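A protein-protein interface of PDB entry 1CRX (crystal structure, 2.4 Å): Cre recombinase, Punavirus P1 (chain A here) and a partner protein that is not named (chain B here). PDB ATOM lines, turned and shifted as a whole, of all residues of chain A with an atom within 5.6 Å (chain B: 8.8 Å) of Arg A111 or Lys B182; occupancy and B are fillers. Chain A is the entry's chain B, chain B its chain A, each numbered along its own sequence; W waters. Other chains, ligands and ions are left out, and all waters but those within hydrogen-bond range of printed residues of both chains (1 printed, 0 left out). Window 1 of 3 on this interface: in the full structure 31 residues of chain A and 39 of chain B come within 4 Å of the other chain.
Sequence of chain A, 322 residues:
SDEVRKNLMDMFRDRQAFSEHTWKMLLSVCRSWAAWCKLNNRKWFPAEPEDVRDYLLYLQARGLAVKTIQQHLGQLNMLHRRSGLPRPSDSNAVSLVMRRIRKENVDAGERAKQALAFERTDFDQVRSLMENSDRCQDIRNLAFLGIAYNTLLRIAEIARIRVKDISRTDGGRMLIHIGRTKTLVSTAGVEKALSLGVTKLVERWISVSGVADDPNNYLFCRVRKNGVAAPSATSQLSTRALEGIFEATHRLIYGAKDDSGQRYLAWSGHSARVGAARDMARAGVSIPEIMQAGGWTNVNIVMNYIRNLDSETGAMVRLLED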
ATOM      1  N   ASN A 105       0.025  -7.362   3.860  1.00  0.00           N
ATOM      2  CA  ASN A 105      -0.844  -7.271   2.692  1.00  0.00           C
ATOM      3  C   ASN A 105      -2.289  -7.457   3.093  1.00  0.00           C
ATOM      4  O   ASN A 105      -3.162  -6.736   2.614  1.00  0.00           O
ATOM      5  CB  ASN A 105      -0.461  -8.323   1.643  1.00  0.00           C
ATOM      6  CG  ASN A 105       0.696  -7.879   0.770  1.00  0.00           C
ATOM      7  OD1 ASN A 105       1.630  -7.210   1.238  1.00  0.00           O
ATOM      8  ND2 ASN A 105       0.651  -8.252  -0.506  1.00  0.00           N
ATOM      9  N   VAL A 106      -2.542  -8.425   3.974  1.00  0.00           N
ATOM     10  CA  VAL A 106      -3.901  -8.686   4.430  1.00  0.00           C
ATOM     11  C   VAL A 106      -4.398  -7.518   5.272  1.00  0.00           C
ATOM     12  O   VAL A 106      -5.544  -7.083   5.139  1.00  0.00           O
ATOM     13  CB  VAL A 106      -3.964  -9.983   5.239  1.00  0.00           C
ATOM     14  CG1 VAL A 106      -5.218 -10.008   6.111  1.00  0.00           C
ATOM     15  CG2 VAL A 106      -3.951 -11.172   4.286  1.00  0.00           C
ATOM     16  N   ASP A 107      -3.518  -7.006   6.128  1.00  0.00           N
ATOM     17  CA  ASP A 107      -3.828  -5.873   7.000  1.00  0.00           C
ATOM     18  C   ASP A 107      -4.287  -4.683   6.178  1.00  0.00           C
ATOM     19  O   ASP A 107      -5.164  -3.936   6.592  1.00  0.00           O
ATOM     20  CB  ASP A 107      -2.589  -5.443   7.778  1.00  0.00           C
ATOM     21  CG  ASP A 107      -2.342  -6.288   8.997  1.00  0.00           C
ATOM     22  OD1 ASP A 107      -3.171  -7.188   9.271  1.00  0.00           O
ATOM     23  OD2 ASP A 107      -1.313  -6.045   9.675  1.00  0.00           O
ATOM     24  N   GLY A 109      -5.811  -4.878   3.538  1.00  0.00           N
ATOM     25  CA  GLY A 109      -7.010  -5.254   2.809  1.00  0.00           C
ATOM     26  C   GLY A 109      -6.971  -6.269   1.682  1.00  0.00           C
ATOM     27  O   GLY A 109      -8.008  -6.557   1.083  1.00  0.00           O
ATOM     28  N   GLU A 110      -5.808  -6.825   1.372  1.00  0.00           N
ATOM     29  CA  GLU A 110      -5.761  -7.792   0.296  1.00  0.00           C
ATOM     30  C   GLU A 110      -6.580  -9.012   0.640  1.00  0.00           C
ATOM     31  O   GLU A 110      -6.532  -9.515   1.761  1.00  0.00           O
ATOM     32  CB  GLU A 110      -4.338  -8.235  -0.012  1.00  0.00           C
ATOM     33  CG  GLU A 110      -4.315  -9.404  -0.997  1.00  0.00           C
ATOM     34  CD  GLU A 110      -2.926  -9.792  -1.428  1.00  0.00           C
ATOM     35  OE1 GLU A 110      -2.034  -8.924  -1.402  1.00  0.00           O
ATOM     36  OE2 GLU A 110      -2.730 -10.968  -1.793  1.00  0.00           O
ATOM     37  N   ARG A 111      -7.329  -9.480  -0.350  1.00  0.00           N
ATOM     38  CA  ARG A 111      -8.170 -10.656  -0.210  1.00  0.00           C
ATOM     39  C   ARG A 111      -8.047 -11.431  -1.502  1.00  0.00           C
ATOM     40  O   ARG A 111      -8.013 -10.842  -2.584  1.00  0.00           O
ATOM     41  CB  ARG A 111      -9.630 -10.252  -0.011  1.00  0.00           C
ATOM     42  CG  ARG A 111     -10.170 -10.370   1.410  1.00  0.00           C
ATOM     43  CD  ARG A 111      -9.100 -10.688   2.429  1.00  0.00           C
ATOM     44  NE  ARG A 111      -9.516 -10.306   3.772  1.00  0.00           N
ATOM     45  CZ  ARG A 111      -9.003  -9.285   4.451  1.00  0.00           C
ATOM     46  NH1 ARG A 111      -8.047  -8.539   3.909  1.00  0.00           N
ATOM     47  NH2 ARG A 111      -9.447  -9.013   5.671  1.00  0.00           N
ATOM     48  N   ALA A 112      -7.960 -12.749  -1.393  1.00  0.00           N
ATOM     49  CA  ALA A 112      -7.869 -13.586  -2.580  1.00  0.00           C
ATOM     50  C   ALA A 112      -9.257 -13.550  -3.204  1.00  0.00           C
ATOM     51  O   ALA A 112     -10.220 -13.977  -2.574  1.00  0.00           O
ATOM     52  CB  ALA A 112      -7.499 -15.011  -2.191  1.00  0.00           C
ATOM     53  N   LYS A 113      -9.364 -13.032  -4.427  1.00  0.00           N
ATOM     54  CA  LYS A 113     -10.663 -12.939  -5.100  1.00  0.00           C
ATOM     55  C   LYS A 113     -11.203 -14.287  -5.555  1.00  0.00           C
ATOM     56  O   LYS A 113     -10.633 -15.340  -5.271  1.00  0.00           O
ATOM     57  CB  LYS A 113     -10.600 -11.995  -6.309  1.00  0.00           C
ATOM     58  CG  LYS A 113      -9.280 -11.278  -6.495  1.00  0.00           C
ATOM     59  CD  LYS A 113      -9.479  -9.912  -7.118  1.00  0.00           C
ATOM     60  CE  LYS A 113      -8.571  -8.882  -6.458  1.00  0.00           C
ATOM     61  NZ  LYS A 113      -9.085  -7.488  -6.581  1.00  0.00           N
ATOM     62  N   ARG B 154     -17.347  -6.842  17.242  1.00  0.00           N
ATOM     63  CA  ARG B 154     -16.445  -6.968  18.377  1.00  0.00           C
ATOM     64  C   ARG B 154     -16.054  -5.563  18.833  1.00  0.00           C
ATOM     65  O   ARG B 154     -16.238  -4.594  18.088  1.00  0.00           O
ATOM     66  CB  ARG B 154     -15.225  -7.804  17.974  1.00  0.00           C
ATOM     67  CG  ARG B 154     -15.541  -9.118  17.328  1.00  0.00           C
ATOM     68  CD  ARG B 154     -14.264  -9.850  16.976  1.00  0.00           C
ATOM     69  NE  ARG B 154     -14.522 -11.128  16.357  1.00  0.00           N
ATOM     70  CZ  ARG B 154     -14.595 -11.312  15.046  1.00  0.00           C
ATOM     71  NH1 ARG B 154     -14.417 -10.292  14.197  1.00  0.00           N
ATOM     72  NH2 ARG B 154     -14.845 -12.495  14.483  1.00  0.00           N
ATOM     73  N   GLU B 157     -13.710  -3.527  16.786  1.00  0.00           N
ATOM     74  CA  GLU B 157     -14.388  -3.169  15.542  1.00  0.00           C
ATOM     75  C   GLU B 157     -15.283  -1.940  15.708  1.00  0.00           C
ATOM     76  O   GLU B 157     -15.307  -1.055  14.844  1.00  0.00           O
ATOM     77  CB  GLU B 157     -15.202  -4.370  15.030  1.00  0.00           C
ATOM     78  CG  GLU B 157     -14.349  -5.425  14.304  1.00  0.00           C
ATOM     79  CD  GLU B 157     -15.006  -6.800  14.197  1.00  0.00           C
ATOM     80  OE1 GLU B 157     -16.243  -6.909  14.364  1.00  0.00           O
ATOM     81  OE2 GLU B 157     -14.271  -7.780  13.937  1.00  0.00           O
ATOM     82  N   ARG B 160     -13.166   1.218  15.762  1.00  0.00           N
ATOM     83  CA  ARG B 160     -12.645   1.716  14.489  1.00  0.00           C
ATOM     84  C   ARG B 160     -13.662   2.351  13.550  1.00  0.00           C
ATOM     85  O   ARG B 160     -13.294   2.942  12.533  1.00  0.00           O
ATOM     86  CB  ARG B 160     -11.911   0.587  13.756  1.00  0.00           C
ATOM     87  CG  ARG B 160     -10.938  -0.184  14.643  1.00  0.00           C
ATOM     88  CD  ARG B 160     -10.120  -1.233  13.869  1.00  0.00           C
ATOM     89  NE  ARG B 160     -10.915  -1.969  12.882  1.00  0.00           N
ATOM     90  CZ  ARG B 160     -11.264  -3.249  12.999  1.00  0.00           C
ATOM     91  NH1 ARG B 160     -10.893  -3.951  14.065  1.00  0.00           N
ATOM     92  NH2 ARG B 160     -11.996  -3.829  12.052  1.00  0.00           N
ATOM     93  N   ILE B 178     -18.170  -2.048   7.495  1.00  0.00           N
ATOM     94  CA  ILE B 178     -17.156  -2.415   8.466  1.00  0.00           C
ATOM     95  C   ILE B 178     -16.302  -3.577   7.976  1.00  0.00           C
ATOM     96  O   ILE B 178     -16.660  -4.253   7.018  1.00  0.00           O
ATOM     97  CB  ILE B 178     -17.835  -2.780   9.830  1.00  0.00           C
ATOM     98  CG1 ILE B 178     -16.776  -2.955  10.918  1.00  0.00           C
ATOM     99  CG2 ILE B 178     -18.675  -4.039   9.691  1.00  0.00           C
ATOM    100  CD1 ILE B 178     -15.911  -1.719  11.137  1.00  0.00           C
ATOM    101  N   GLY B 179     -15.162  -3.786   8.631  1.00  0.00           N
ATOM    102  CA  GLY B 179     -14.277  -4.885   8.283  1.00  0.00           C
ATOM    103  C   GLY B 179     -14.109  -5.827   9.471  1.00  0.00           C
ATOM    104  O   GLY B 179     -13.550  -5.430  10.498  1.00  0.00           O
ATOM    105  N   ARG B 180     -14.599  -7.064   9.350  1.00  0.00           N
ATOM    106  CA  ARG B 180     -14.484  -8.039  10.439  1.00  0.00           C
ATOM    107  C   ARG B 180     -13.667  -9.300  10.125  1.00  0.00           C
ATOM    108  O   ARG B 180     -13.814 -10.311  10.811  1.00  0.00           O
ATOM    109  CB  ARG B 180     -15.870  -8.470  10.953  1.00  0.00           C
ATOM    110  CG  ARG B 180     -17.073  -7.963  10.171  1.00  0.00           C
ATOM    111  CD  ARG B 180     -17.916  -9.136   9.651  1.00  0.00           C
ATOM    112  NE  ARG B 180     -19.195  -9.295  10.346  1.00  0.00           N
ATOM    113  CZ  ARG B 180     -20.139 -10.166   9.992  1.00  0.00           C
ATOM    114  NH1 ARG B 180     -19.959 -10.965   8.952  1.00  0.00           N
ATOM    115  NH2 ARG B 180     -21.265 -10.240  10.683  1.00  0.00           N
ATOM    116  N   THR B 181     -12.826  -9.252   9.093  1.00  0.00           N
ATOM    117  CA  THR B 181     -11.984 -10.403   8.746  1.00  0.00           C
ATOM    118  C   THR B 181     -10.508  -9.997   8.722  1.00  0.00           C
ATOM    119  O   THR B 181     -10.174  -8.823   8.530  1.00  0.00           O
ATOM    120  CB  THR B 181     -12.341 -11.014   7.364  1.00  0.00           C
ATOM    121  OG1 THR B 181     -12.149 -10.034   6.338  1.00  0.00           O
ATOM    122  CG2 THR B 181     -13.776 -11.512   7.349  1.00  0.00           C
ATOM    123  N   LYS B 182      -9.627 -10.969   8.922  1.00  0.00           N
ATOM    124  CA  LYS B 182      -8.196 -10.694   8.940  1.00  0.00           C
ATOM    125  C   LYS B 182      -7.386 -11.801   8.270  1.00  0.00           C
ATOM    126  O   LYS B 182      -6.228 -12.034   8.609  1.00  0.00           O
ATOM    127  CB  LYS B 182      -7.723 -10.499  10.385  1.00  0.00           C
ATOM    128  CG  LYS B 182      -8.847 -10.390  11.417  1.00  0.00           C
ATOM    129  CD  LYS B 182      -8.814 -11.555  12.404  1.00  0.00           C
ATOM    130  CE  LYS B 182      -9.663 -12.726  11.921  1.00  0.00           C
ATOM    131  NZ  LYS B 182      -9.098 -14.040  12.348  1.00  0.00           N
ATOM    132  N   THR B 183      -8.007 -12.488   7.318  1.00  0.00           N
ATOM    133  CA  THR B 183      -7.336 -13.556   6.592  1.00  0.00           C
ATOM    134  C   THR B 183      -7.440 -13.295   5.091  1.00  0.00           C
ATOM    135  O   THR B 183      -8.380 -12.651   4.622  1.00  0.00           O
ATOM    136  CB  THR B 183      -7.953 -14.920   6.917  1.00  0.00           C
ATOM    137  OG1 THR B 183      -9.328 -14.927   6.520  1.00  0.00           O
ATOM    138  CG2 THR B 183      -7.864 -15.197   8.403  1.00  0.00           C
ATOM    139  N   LEU B 184      -6.461 -13.788   4.344  1.00  0.00           N
ATOM    140  CA  LEU B 184      -6.423 -13.596   2.905  1.00  0.00           C
ATOM    141  C   LEU B 184      -7.689 -14.121   2.243  1.00  0.00           C
ATOM    142  O   LEU B 184      -8.349 -13.414   1.481  1.00  0.00           O
ATOM    143  CB  LEU B 184      -5.204 -14.310   2.327  1.00  0.00           C
ATOM    144  CG  LEU B 184      -4.889 -13.999   0.869  1.00  0.00           C
ATOM    145  CD1 LEU B 184      -4.548 -12.520   0.712  1.00  0.00           C
ATOM    146  CD2 LEU B 184      -3.738 -14.884   0.426  1.00  0.00           C
ATOM    147  N   VAL B 185      -8.024 -15.370   2.529  1.00  0.00           N
ATOM    148  CA  VAL B 185      -9.214 -15.964   1.950  1.00  0.00           C
ATOM    149  C   VAL B 185     -10.385 -15.695   2.876  1.00  0.00           C
ATOM    150  O   VAL B 185     -10.718 -16.513   3.736  1.00  0.00           O
ATOM    151  CB  VAL B 185      -9.035 -17.481   1.759  1.00  0.00           C
ATOM    152  CG1 VAL B 185     -10.171 -18.032   0.938  1.00  0.00           C
ATOM    153  CG2 VAL B 185      -7.709 -17.760   1.073  1.00  0.00           C
ATOM    154  N   SER B 186     -10.997 -14.531   2.701  1.00  0.00           N
ATOM    155  CA  SER B 186     -12.132 -14.120   3.518  1.00  0.00           C
ATOM    156  C   SER B 186     -12.783 -12.891   2.896  1.00  0.00           C
ATOM    157  O   SER B 186     -12.313 -12.380   1.881  1.00  0.00           O
ATOM    158  CB  SER B 186     -11.671 -13.793   4.939  1.00  0.00           C
ATOM    159  OG  SER B 186     -11.363 -12.415   5.065  1.00  0.00           O
ATOM    160  N   THR B 187     -13.861 -12.415   3.507  1.00  0.00           N
ATOM    161  CA  THR B 187     -14.555 -11.244   2.985  1.00  0.00           C
ATOM    162  C   THR B 187     -13.914  -9.955   3.505  1.00  0.00           C
ATOM    163  O   THR B 187     -13.848  -9.723   4.713  1.00  0.00           O
ATOM    164  CB  THR B 187     -16.060 -11.272   3.361  1.00  0.00           C
ATOM    165  OG1 THR B 187     -16.273 -10.502   4.549  1.00  0.00           O
ATOM    166  CG2 THR B 187     -16.526 -12.707   3.601  1.00  0.00           C
ATOM    167  N   ALA B 188     -13.439  -9.126   2.579  1.00  0.00           N
ATOM    168  CA  ALA B 188     -12.789  -7.862   2.914  1.00  0.00           C
ATOM    169  C   ALA B 188     -13.618  -6.984   3.849  1.00  0.00           C
ATOM    170  O   ALA B 188     -13.077  -6.299   4.718  1.00  0.00           O
ATOM    171  CB  ALA B 188     -12.463  -7.097   1.634  1.00  0.00           C
ATOM    172  N   GLY B 189     -14.932  -6.996   3.667  1.00  0.00           N
ATOM    173  CA  GLY B 189     -15.787  -6.189   4.516  1.00  0.00           C
ATOM    174  C   GLY B 189     -17.239  -6.598   4.431  1.00  0.00           C
ATOM    175  O   GLY B 189     -17.631  -7.391   3.575  1.00  0.00           O
ATOM    176  N   GLY B 295     -20.302 -13.446  12.023  1.00  0.00           N
ATOM    177  CA  GLY B 295     -19.135 -13.662  11.194  1.00  0.00           C
ATOM    178  C   GLY B 295     -18.454 -14.995  11.456  1.00  0.00           C
ATOM    179  O   GLY B 295     -17.247 -15.121  11.284  1.00  0.00           O
HETATM  180  O   HOH W   1      -7.643  -7.083   7.261  1.00  0.00           O
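The side-chain hydroxyl of Ser B186 lies within hydrogen-bond range of the side-chain hydroxyl of Thr B181 (2.8 Å). The side-chain hydroxyl (OG1) of Thr B183 lies within hydrogen-bond range of the backbone carbonyl oxygen (O) of Val B185 (3.5 Å). The backbone carbonyl oxygen (O) of Thr B183 is in hydrogen-bond range of the side-chain hydroxyl (OG) of Ser B186. The side-chain amide nitrogen of Asn A105 is in hydrogen-bond range of the side-chain carboxylate of Glu A110. The backbone carbonyl oxygen (O) of Val A106 sits at hydrogen-bond distance from the guanidinium group (NH1) of Arg A111 (3.1 Å). The backbone carbonyl oxygen (O) of Gly A109 lies close to the guanidinium group (NH1) of Arg A111 (3.5 Å).
Lys B182 touches Val A106 (O to CG1, 3.4 Å). Thr B183 touches Val A106 (N to CG1, 3.9 Å). N of Leu B184 touches CG2 of Val A106, 3.6 Å away. Glu A110 touches Leu B184 (OE2 to CD1, 3.5 Å). Lys B182 touches Arg A111. Leu B184 touches Arg A111. N of Ala B188 touches CG of Arg A111 (3.7 Å).
Water W1 lies within hydrogen-bond range of O of Val A106, NH2 of Arg A111 and O of Thr B181.
O of Thr B181 lies within hydrogen-bond range of NH2 of Arg A111 (3.0 Å). The guanidinium group of Arg A111 sits at hydrogen-bond distance from the backbone carbonyl oxygen of Thr B183, 2.7 Å away. The backbone carbonyl oxygen (O) of Leu B184 sits at hydrogen-bond distance from the backbone NH (N) of Ala A112. The side-chain hydroxyl (OG) of Ser B186 is in hydrogen-bond range of the guanidinium group (NE) of Arg A111, at 3.1 Å.
Arg A111 touches just these residues of chain B: Thr B181, Lys B182, Thr B183, Leu B184, Ser B186 and Ala B188. Lys B182 touches just these residues of chain A: Val A106 and Arg A111. No residue of chain B comes within 4 Å of Gly A109. Ala A112 touches just one residue of chain B: Leu B184 (3.0 Å). Printed residues of chain A within 4 Å of Leu B184: Val A106 (3.6 Å), Glu A110 (3.5 Å), Arg A111 (3.0 Å) and Ala A112 (3.0 Å). Of the printed residues of chain B, Glu A110 touches Leu B184. Of the printed residues of chain A, Ala B188 touches Arg A111 (3.7 Å). Printed residues of chain A within 4 Å of Thr B181: Arg A111 (3.0 Å). Of the printed residues of chain B, Val A106 touches Lys B182, Thr B183 and Leu B184. The nearest residue of chain B that does not touch Arg A111 is Thr B187 (4.3 Å). The nearest printed residue of chain A that does not touch Lys B182 is Asp A107 (5.7 Å).
Of the 16 printed residues of chain B, 6 touch a printed residue of chain A. Of the 8 printed residues of chain A, 4 touch a printed residue of chain B. Hydrophobic or aromatic side chains of chain A that line the printed part of chain B: Val A106.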
